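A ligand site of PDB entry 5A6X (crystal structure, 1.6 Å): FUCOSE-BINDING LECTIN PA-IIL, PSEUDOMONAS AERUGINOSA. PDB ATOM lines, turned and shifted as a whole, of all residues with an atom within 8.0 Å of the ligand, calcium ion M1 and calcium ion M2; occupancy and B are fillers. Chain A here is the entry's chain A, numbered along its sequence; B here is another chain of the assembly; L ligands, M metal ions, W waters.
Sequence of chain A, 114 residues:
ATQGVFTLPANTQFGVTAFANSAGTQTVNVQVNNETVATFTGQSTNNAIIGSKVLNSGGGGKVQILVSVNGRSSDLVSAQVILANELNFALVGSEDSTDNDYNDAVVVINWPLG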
ATOM      1  N   ALA A  20      29.350  10.981 -21.951  1.00  0.00           N
ATOM      2  CA  ALA A  20      30.023  11.360 -23.190  1.00  0.00           C
ATOM      3  C   ALA A  20      29.234  10.929 -24.424  1.00  0.00           C
ATOM      4  O   ALA A  20      28.656   9.853 -24.473  1.00  0.00           O
ATOM      5  CB  ALA A  20      31.429  10.791 -23.280  1.00  0.00           C
ATOM      6  N   ASN A  21      29.241  11.829 -25.426  1.00  0.00           N
ATOM      7  CA  ASN A  21      28.582  11.592 -26.721  1.00  0.00           C
ATOM      8  C   ASN A  21      29.335  12.305 -27.811  1.00  0.00           C
ATOM      9  O   ASN A  21      28.850  13.284 -28.386  1.00  0.00           O
ATOM     10  CB  ASN A  21      27.118  12.123 -26.705  1.00  0.00           C
ATOM     11  CG  ASN A  21      26.222  11.339 -25.785  1.00  0.00           C
ATOM     12  OD1 ASN A  21      25.740  10.270 -26.155  1.00  0.00           O
ATOM     13  ND2 ASN A  21      25.957  11.902 -24.595  1.00  0.00           N
ATOM     14  N   SER A  22      30.523  11.779 -28.129  1.00  0.00           N
ATOM     15  CA  SER A  22      31.409  12.414 -29.101  1.00  0.00           C
ATOM     16  C   SER A  22      32.508  11.460 -29.544  1.00  0.00           C
ATOM     17  O   SER A  22      32.937  10.618 -28.778  1.00  0.00           O
ATOM     18  CB  SER A  22      32.028  13.655 -28.494  1.00  0.00           C
ATOM     19  OG  SER A  22      32.963  14.246 -29.377  1.00  0.00           O
ATOM     20  N   ALA A  23      33.027  11.701 -30.738  1.00  0.00           N
ATOM     21  CA  ALA A  23      34.237  10.997 -31.155  1.00  0.00           C
ATOM     22  C   ALA A  23      35.440  11.428 -30.327  1.00  0.00           C
ATOM     23  O   ALA A  23      36.403  10.660 -30.183  1.00  0.00           O
ATOM     24  CB  ALA A  23      34.488  11.290 -32.616  1.00  0.00           C
ATOM     25  N   GLY A  24      35.422  12.624 -29.788  1.00  0.00           N
ATOM     26  CA  GLY A  24      36.573  13.175 -29.025  1.00  0.00           C
ATOM     27  C   GLY A  24      36.608  12.704 -27.603  1.00  0.00           C
ATOM     28  O   GLY A  24      35.525  12.570 -26.965  1.00  0.00           O
ATOM     29  N   GLN A  26      36.688  13.295 -23.896  1.00  0.00           N
ATOM     30  CA  GLN A  26      36.242  14.409 -23.041  1.00  0.00           C
ATOM     31  C   GLN A  26      37.020  14.462 -21.732  1.00  0.00           C
ATOM     32  O   GLN A  26      37.244  13.440 -21.108  1.00  0.00           O
ATOM     33  CB  GLN A  26      34.766  14.245 -22.683  1.00  0.00           C
ATOM     34  CG  GLN A  26      33.853  14.061 -23.912  1.00  0.00           C
ATOM     35  CD  GLN A  26      33.801  15.290 -24.787  1.00  0.00           C
ATOM     36  OE1 GLN A  26      33.575  16.401 -24.308  1.00  0.00           O
ATOM     37  NE2 GLN A  26      34.054  15.112 -26.069  1.00  0.00           N
ATOM     38  N   GLN A  43      35.634   8.524 -23.245  1.00  0.00           N
ATOM     39  CA  GLN A  43      35.155   8.628 -24.605  1.00  0.00           C
ATOM     40  C   GLN A  43      34.006   7.672 -24.844  1.00  0.00           C
ATOM     41  O   GLN A  43      34.064   6.507 -24.453  1.00  0.00           O
ATOM     42  CB  GLN A  43      36.273   8.418 -25.633  1.00  0.00           C
ATOM     43  CG  GLN A  43      35.872   8.660 -27.106  1.00  0.00           C
ATOM     44  CD  GLN A  43      35.066   7.552 -27.743  1.00  0.00           C
ATOM     45  OE1 GLN A  43      35.343   6.361 -27.535  1.00  0.00           O
ATOM     46  NE2 GLN A  43      34.101   7.922 -28.604  1.00  0.00           N
ATOM     47  N   SER A  44      32.948   8.179 -25.475  1.00  0.00           N
ATOM     48  CA  SER A  44      31.792   7.370 -25.840  1.00  0.00           C
ATOM     49  C   SER A  44      30.975   8.140 -26.847  1.00  0.00           C
ATOM     50  O   SER A  44      30.915   9.367 -26.751  1.00  0.00           O
ATOM     51  CB  SER A  44      30.909   7.082 -24.631  1.00  0.00           C
ATOM     52  OG  SER A  44      29.766   6.299 -24.939  1.00  0.00           O
ATOM     53  N   THR A  45      30.368   7.430 -27.804  1.00  0.00           N
ATOM     54  CA  THR A  45      29.296   8.012 -28.623  1.00  0.00           C
ATOM     55  C   THR A  45      27.922   7.489 -28.238  1.00  0.00           C
ATOM     56  O   THR A  45      26.941   7.654 -29.001  1.00  0.00           O
ATOM     57  CB  THR A  45      29.569   7.806 -30.108  1.00  0.00           C
ATOM     58  OG1 THR A  45      29.800   6.418 -30.350  1.00  0.00           O
ATOM     59  CG2 THR A  45      30.702   8.654 -30.590  1.00  0.00           C
ATOM     60  N   ASN A  46      27.815   6.890 -27.076  1.00  0.00           N
ATOM     61  CA  ASN A  46      26.580   6.250 -26.636  1.00  0.00           C
ATOM     62  C   ASN A  46      26.245   6.494 -25.184  1.00  0.00           C
ATOM     63  O   ASN A  46      25.687   5.658 -24.475  1.00  0.00           O
ATOM     64  CB  ASN A  46      26.564   4.747 -26.947  1.00  0.00           C
ATOM     65  CG  ASN A  46      25.135   4.229 -27.063  1.00  0.00           C
ATOM     66  OD1 ASN A  46      24.218   4.973 -27.473  1.00  0.00           O
ATOM     67  ND2 ASN A  46      24.924   3.029 -26.624  1.00  0.00           N
ATOM     68  N   VAL A  69      38.614  19.097 -24.846  1.00  0.00           N
ATOM     69  CA  VAL A  69      38.945  17.960 -25.700  1.00  0.00           C
ATOM     70  C   VAL A  69      40.339  18.239 -26.181  1.00  0.00           C
ATOM     71  O   VAL A  69      40.501  19.189 -26.926  1.00  0.00           O
ATOM     72  CB  VAL A  69      37.939  17.788 -26.829  1.00  0.00           C
ATOM     73  CG1 VAL A  69      38.340  16.621 -27.769  1.00  0.00           C
ATOM     74  CG2 VAL A  69      36.556  17.550 -26.256  1.00  0.00           C
ATOM     75  N   SER A  94      27.844  20.687 -23.495  1.00  0.00           N
ATOM     76  CA  SER A  94      29.074  21.223 -24.087  1.00  0.00           C
ATOM     77  C   SER A  94      29.173  20.777 -25.533  1.00  0.00           C
ATOM     78  O   SER A  94      28.719  19.705 -25.908  1.00  0.00           O
ATOM     79  CB  SER A  94      30.270  20.748 -23.258  1.00  0.00           C
ATOM     80  OG  SER A  94      30.507  19.354 -23.322  1.00  0.00           O
ATOM     81  N   GLU A  95      29.826  21.642 -26.301  1.00  0.00           N
ATOM     82  CA  GLU A  95      30.026  21.412 -27.734  1.00  0.00           C
ATOM     83  C   GLU A  95      31.505  21.514 -28.097  1.00  0.00           C
ATOM     84  O   GLU A  95      32.130  22.577 -27.881  1.00  0.00           O
ATOM     85  CB  GLU A  95      29.213  22.414 -28.544  1.00  0.00           C
ATOM     86  CG  GLU A  95      29.381  22.278 -30.052  1.00  0.00           C
ATOM     87  CD  GLU A  95      29.021  20.913 -30.574  1.00  0.00           C
ATOM     88  OE1 GLU A  95      27.932  20.365 -30.199  1.00  0.00           O
ATOM     89  OE2 GLU A  95      29.866  20.297 -31.293  1.00  0.00           O
ATOM     90  N   ASP A  96      32.025  20.440 -28.686  1.00  0.00           N
ATOM     91  CA  ASP A  96      33.429  20.299 -29.039  1.00  0.00           C
ATOM     92  C   ASP A  96      33.720  20.494 -30.537  1.00  0.00           C
ATOM     93  O   ASP A  96      34.881  20.442 -30.950  1.00  0.00           O
ATOM     94  CB  ASP A  96      34.023  19.024 -28.482  1.00  0.00           C
ATOM     95  CG  ASP A  96      33.495  17.772 -29.146  1.00  0.00           C
ATOM     96  OD1 ASP A  96      33.051  17.819 -30.303  1.00  0.00           O
ATOM     97  OD2 ASP A  96      33.600  16.697 -28.542  1.00  0.00           O
ATOM     98  N   SER A  97      32.656  20.735 -31.315  1.00  0.00           N
ATOM     99  CA  SER A  97      32.817  20.747 -32.787  1.00  0.00           C
ATOM    100  C   SER A  97      31.806  21.707 -33.373  1.00  0.00           C
ATOM    101  O   SER A  97      31.583  22.751 -32.814  1.00  0.00           O
ATOM    102  CB  SER A  97      32.690  19.319 -33.299  1.00  0.00           C
ATOM    103  OG  SER A  97      33.023  19.217 -34.685  1.00  0.00           O
ATOM    104  N   THR A  98      31.140  21.293 -34.458  1.00  0.00           N
ATOM    105  CA  THR A  98      30.332  22.215 -35.222  1.00  0.00           C
ATOM    106  C   THR A  98      28.895  21.819 -35.463  1.00  0.00           C
ATOM    107  O   THR A  98      28.113  22.615 -36.015  1.00  0.00           O
ATOM    108  CB  THR A  98      30.953  22.414 -36.643  1.00  0.00           C
ATOM    109  OG1 THR A  98      31.088  21.161 -37.257  1.00  0.00           O
ATOM    110  CG2 THR A  98      32.304  23.073 -36.530  1.00  0.00           C
ATOM    111  N   ASP A  99      28.489  20.652 -34.973  1.00  0.00           N
ATOM    112  CA  ASP A  99      27.068  20.221 -35.177  1.00  0.00           C
ATOM    113  C   ASP A  99      26.071  20.780 -34.217  1.00  0.00           C
ATOM    114  O   ASP A  99      24.884  20.673 -34.445  1.00  0.00           O
ATOM    115  CB  ASP A  99      26.975  18.691 -35.264  1.00  0.00           C
ATOM    116  CG  ASP A  99      27.280  17.974 -33.965  1.00  0.00           C
ATOM    117  OD1 ASP A  99      27.946  18.597 -33.080  1.00  0.00           O
ATOM    118  OD2 ASP A  99      26.936  16.770 -33.896  1.00  0.00           O
ATOM    119  N   ASN A 100      26.563  21.352 -33.121  1.00  0.00           N
ATOM    120  CA  ASN A 100      25.706  22.018 -32.135  1.00  0.00           C
ATOM    121  C   ASN A 100      24.648  21.123 -31.541  1.00  0.00           C
ATOM    122  O   ASN A 100      23.507  21.535 -31.351  1.00  0.00           O
ATOM    123  CB  ASN A 100      25.148  23.305 -32.725  1.00  0.00           C
ATOM    124  CG  ASN A 100      26.243  24.289 -33.030  1.00  0.00           C
ATOM    125  OD1 ASN A 100      27.354  24.187 -32.523  1.00  0.00           O
ATOM    126  ND2 ASN A 100      25.919  25.255 -33.864  1.00  0.00           N
ATOM    127  N   ASP A 101      25.033  19.893 -31.275  1.00  0.00           N
ATOM    128  CA  ASP A 101      24.202  19.038 -30.427  1.00  0.00           C
ATOM    129  C   ASP A 101      24.413  19.294 -28.933  1.00  0.00           C
ATOM    130  O   ASP A 101      23.515  18.976 -28.121  1.00  0.00           O
ATOM    131  CB  ASP A 101      24.269  17.556 -30.782  1.00  0.00           C
ATOM    132  CG  ASP A 101      25.662  16.922 -30.629  1.00  0.00           C
ATOM    133  OD1 ASP A 101      26.634  17.615 -30.308  1.00  0.00           O
ATOM    134  OD2 ASP A 101      25.703  15.668 -30.860  1.00  0.00           O
ATOM    135  N   TYR A 102      25.517  19.903 -28.558  1.00  0.00           N
ATOM    136  CA  TYR A 102      25.746  20.280 -27.138  1.00  0.00           C
ATOM    137  C   TYR A 102      25.697  19.109 -26.144  1.00  0.00           C
ATOM    138  O   TYR A 102      25.552  19.336 -24.956  1.00  0.00           O
ATOM    139  CB  TYR A 102      24.856  21.488 -26.712  1.00  0.00           C
ATOM    140  CG  TYR A 102      25.451  22.781 -27.236  1.00  0.00           C
ATOM    141  CD1 TYR A 102      25.192  23.247 -28.495  1.00  0.00           C
ATOM    142  CD2 TYR A 102      26.374  23.423 -26.476  1.00  0.00           C
ATOM    143  CE1 TYR A 102      25.838  24.422 -28.941  1.00  0.00           C
ATOM    144  CE2 TYR A 102      27.050  24.546 -26.912  1.00  0.00           C
ATOM    145  CZ  TYR A 102      26.748  25.032 -28.153  1.00  0.00           C
ATOM    146  OH  TYR A 102      27.443  26.154 -28.615  1.00  0.00           O
ATOM    147  N   ASN A 103      25.952  17.886 -26.589  1.00  0.00           N
ATOM    148  CA  ASN A 103      25.866  16.689 -25.730  1.00  0.00           C
ATOM    149  C   ASN A 103      27.221  16.024 -25.614  1.00  0.00           C
ATOM    150  O   ASN A 103      27.320  14.914 -25.080  1.00  0.00           O
ATOM    151  CB  ASN A 103      24.841  15.725 -26.273  1.00  0.00           C
ATOM    152  CG  ASN A 103      25.310  15.035 -27.517  1.00  0.00           C
ATOM    153  OD1 ASN A 103      26.375  15.340 -28.041  1.00  0.00           O
ATOM    154  ND2 ASN A 103      24.563  14.074 -27.971  1.00  0.00           N
ATOM    155  N   ASP A 104      28.272  16.710 -26.088  1.00  0.00           N
ATOM    156  CA  ASP A 104      29.527  15.983 -26.274  1.00  0.00           C
ATOM    157  C   ASP A 104      30.151  15.498 -24.920  1.00  0.00           C
ATOM    158  O   ASP A 104      30.612  14.350 -24.802  1.00  0.00           O
ATOM    159  CB  ASP A 104      30.460  16.854 -27.095  1.00  0.00           C
ATOM    160  CG  ASP A 104      29.892  17.194 -28.441  1.00  0.00           C
ATOM    161  OD1 ASP A 104      29.250  16.324 -29.040  1.00  0.00           O
ATOM    162  OD2 ASP A 104      30.147  18.324 -28.910  1.00  0.00           O
ATOM    163  N   ALA A 105      30.045  16.365 -23.922  1.00  0.00           N
ATOM    164  CA  ALA A 105      30.021  15.974 -22.520  1.00  0.00           C
ATOM    165  C   ALA A 105      28.803  16.629 -21.876  1.00  0.00           C
ATOM    166  O   ALA A 105      28.564  17.837 -22.068  1.00  0.00           O
ATOM    167  CB  ALA A 105      31.287  16.396 -21.774  1.00  0.00           C
ATOM    168  N   PRO B 112      19.677  14.995 -27.193  1.00  0.00           N
ATOM    169  CA  PRO B 112      20.051  13.844 -27.988  1.00  0.00           C
ATOM    170  C   PRO B 112      21.291  13.137 -27.487  1.00  0.00           C
ATOM    171  O   PRO B 112      22.070  13.687 -26.691  1.00  0.00           O
ATOM    172  CB  PRO B 112      20.388  14.488 -29.328  1.00  0.00           C
ATOM    173  CG  PRO B 112      20.899  15.814 -28.987  1.00  0.00           C
ATOM    174  CD  PRO B 112      20.015  16.272 -27.854  1.00  0.00           C
ATOM    175  N   LEU B 113      21.500  11.946 -28.028  1.00  0.00           N
ATOM    176  CA  LEU B 113      22.732  11.183 -27.831  1.00  0.00           C
ATOM    177  C   LEU B 113      23.554  11.156 -29.104  1.00  0.00           C
ATOM    178  O   LEU B 113      23.117  11.658 -30.135  1.00  0.00           O
ATOM    179  CB  LEU B 113      22.467   9.764 -27.438  1.00  0.00           C
ATOM    180  CG  LEU B 113      21.537   9.576 -26.271  1.00  0.00           C
ATOM    181  CD1 LEU B 113      21.520   8.100 -25.924  1.00  0.00           C
ATOM    182  CD2 LEU B 113      21.964  10.395 -25.074  1.00  0.00           C
ATOM    183  N   GLY B 114      24.782  10.647 -28.980  1.00  0.00           N
ATOM    184  CA  GLY B 114      25.648  10.474 -30.152  1.00  0.00           C
ATOM    185  C   GLY B 114      26.577  11.608 -30.473  1.00  0.00           C
ATOM    186  O   GLY B 114      26.382  12.762 -30.043  1.00  0.00           O
ATOM    187  OXT GLY B 114      27.521  11.311 -31.267  1.00  0.00           O
HETATM  188  C1  LIG L   1      32.006  15.013 -32.499  1.00  0.00           C
HETATM  189  C2  LIG L   1      30.766  15.616 -31.833  1.00  0.00           C
HETATM  190  C3  LIG L   1      29.547  15.323 -32.652  1.00  0.00           C
HETATM  191  C4  LIG L   1      29.377  13.823 -32.731  1.00  0.00           C
HETATM  192  C5  LIG L   1      30.616  13.198 -33.354  1.00  0.00           C
HETATM  193  C6  LIG L   1      30.609  11.683 -33.430  1.00  0.00           C
HETATM  194  O1  LIG L   1      32.119  15.608 -33.760  1.00  0.00           O
HETATM  195  O2  LIG L   1      30.907  17.021 -31.716  1.00  0.00           O
HETATM  196  O3  LIG L   1      28.440  15.871 -31.883  1.00  0.00           O
HETATM  197  O4  LIG L   1      29.111  13.346 -31.392  1.00  0.00           O
HETATM  198  O5  LIG L   1      31.791  13.625 -32.642  1.00  0.00           O
HETATM  199  C7  LIG L   1      33.335  15.238 -34.414  1.00  0.00           C
HETATM  200 CA    CA M   1      28.827  18.120 -30.923  1.00  0.00          CA
HETATM  201 CA    CA M   2      27.718  14.707 -29.862  1.00  0.00          CA
HETATM  202  O   HOH W   1      30.458  17.841 -35.027  1.00  0.00           O
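OD1 of Asp 96 lies close to O2 of the ligand, at 2.7 Å.
N of Ala 23 is in hydrogen-bond range of O5 of the ligand.
The backbone NH (N) of Asn 21 lies close to the backbone carbonyl oxygen (O) of Ser 44 (3.3 Å).
The side-chain amide nitrogen of Asn 103 is in hydrogen-bond range of the backbone carbonyl oxygen of Pro 112 of chain B (2.8 Å).
OD2 of Asp 104 sits close to N of Asp 96 (2.8 Å).
The backbone carbonyl oxygen of Ser 94 sits at hydrogen-bond distance from the backbone NH of Asp 104 (3.0 Å).
The side-chain carboxylate (OE2) of Glu 95 lies close to the backbone NH (N) of Ser 97, at 2.8 Å.
The side-chain carboxylate (OD2) of Asp 96 lies within hydrogen-bond range of the side-chain amide nitrogen (NE2) of Gln 26.
The side-chain hydroxyl (OG) of Ser 22 is in hydrogen-bond range of the backbone NH (N) of Gly 24, at 3.0 Å.
N of Ser 22 lies within hydrogen-bond range of O of Ser 44 (2.8 Å).
OG of Ser 22 touches C1 of the ligand (3.4 Å).
Ser 97 touches the ligand.
Hydrophobic or aromatic side chains within 4 Å of the ligand: Ala 23.
Of the 26 residues printed, 10 come within 4 Å of the ligand.
Within 4 Å of calcium ion M1: Glu 95, Asp 99, Asp 101 and Asp 104.
The nearest printed residue that does not touch calcium ion M1 is Asp 96 (4.3 Å).
Within 4 Å of calcium ion M2: Asn 21, Asp 101, Asn 103, Asp 104 and Gly 114 of chain B.
The nearest printed residue that does not touch calcium ion M2 is Ser 22 (4.4 Å).
The side-chain carboxylate (OD1) of Asp 101 binds calcium ion M1, at 2.3 Å.
OD1 of Asp 99 is bound to calcium ion M1 (2.4 Å).
The side-chain carboxylate (OD2) of Asp 104 binds calcium ion M1 (2.4 Å).
Calcium ion M1 is bound by the side-chain carboxylate (OE2) of Glu 95 (2.4 Å).
O3 of the ligand is bound to calcium ion M1 (2.5 Å).
O2 of the ligand binds calcium ion M1.
Calcium ion M1 is bound by the side-chain carboxylate (OE1) of Glu 95 (2.5 Å).
The side-chain carboxylate (OD1) of Asp 104 binds calcium ion M1, at 2.6 Å.
O of Asn 21 is bound to calcium ion M2.
OD1 of Asn 103 is bound to calcium ion M2, at 2.3 Å.
The chain-end carboxylate (O) of Gly 114 of chain B binds calcium ion M2, at 2.4 Å.
OD1 of Asp 104 is bound to calcium ion M2 (2.4 Å).
Calcium ion M2 is bound by O3 of the ligand, 2.4 Å away.
Calcium ion M2 is bound by OD2 of Asp 101 (2.4 Å).
O4 of the ligand binds calcium ion M2 (2.5 Å).
Calcium ion M2 has seven donor atoms within binding distance.
Slightly farther from calcium ion M2 lies the side-chain carboxylate (OD1) of Asp 101 (3.1 Å).
Water W1 lies within hydrogen-bond range of OG of Ser 97 (2.9 Å), O1 of the ligand (3.1 Å) and N of Asp 99 (3.4 Å).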
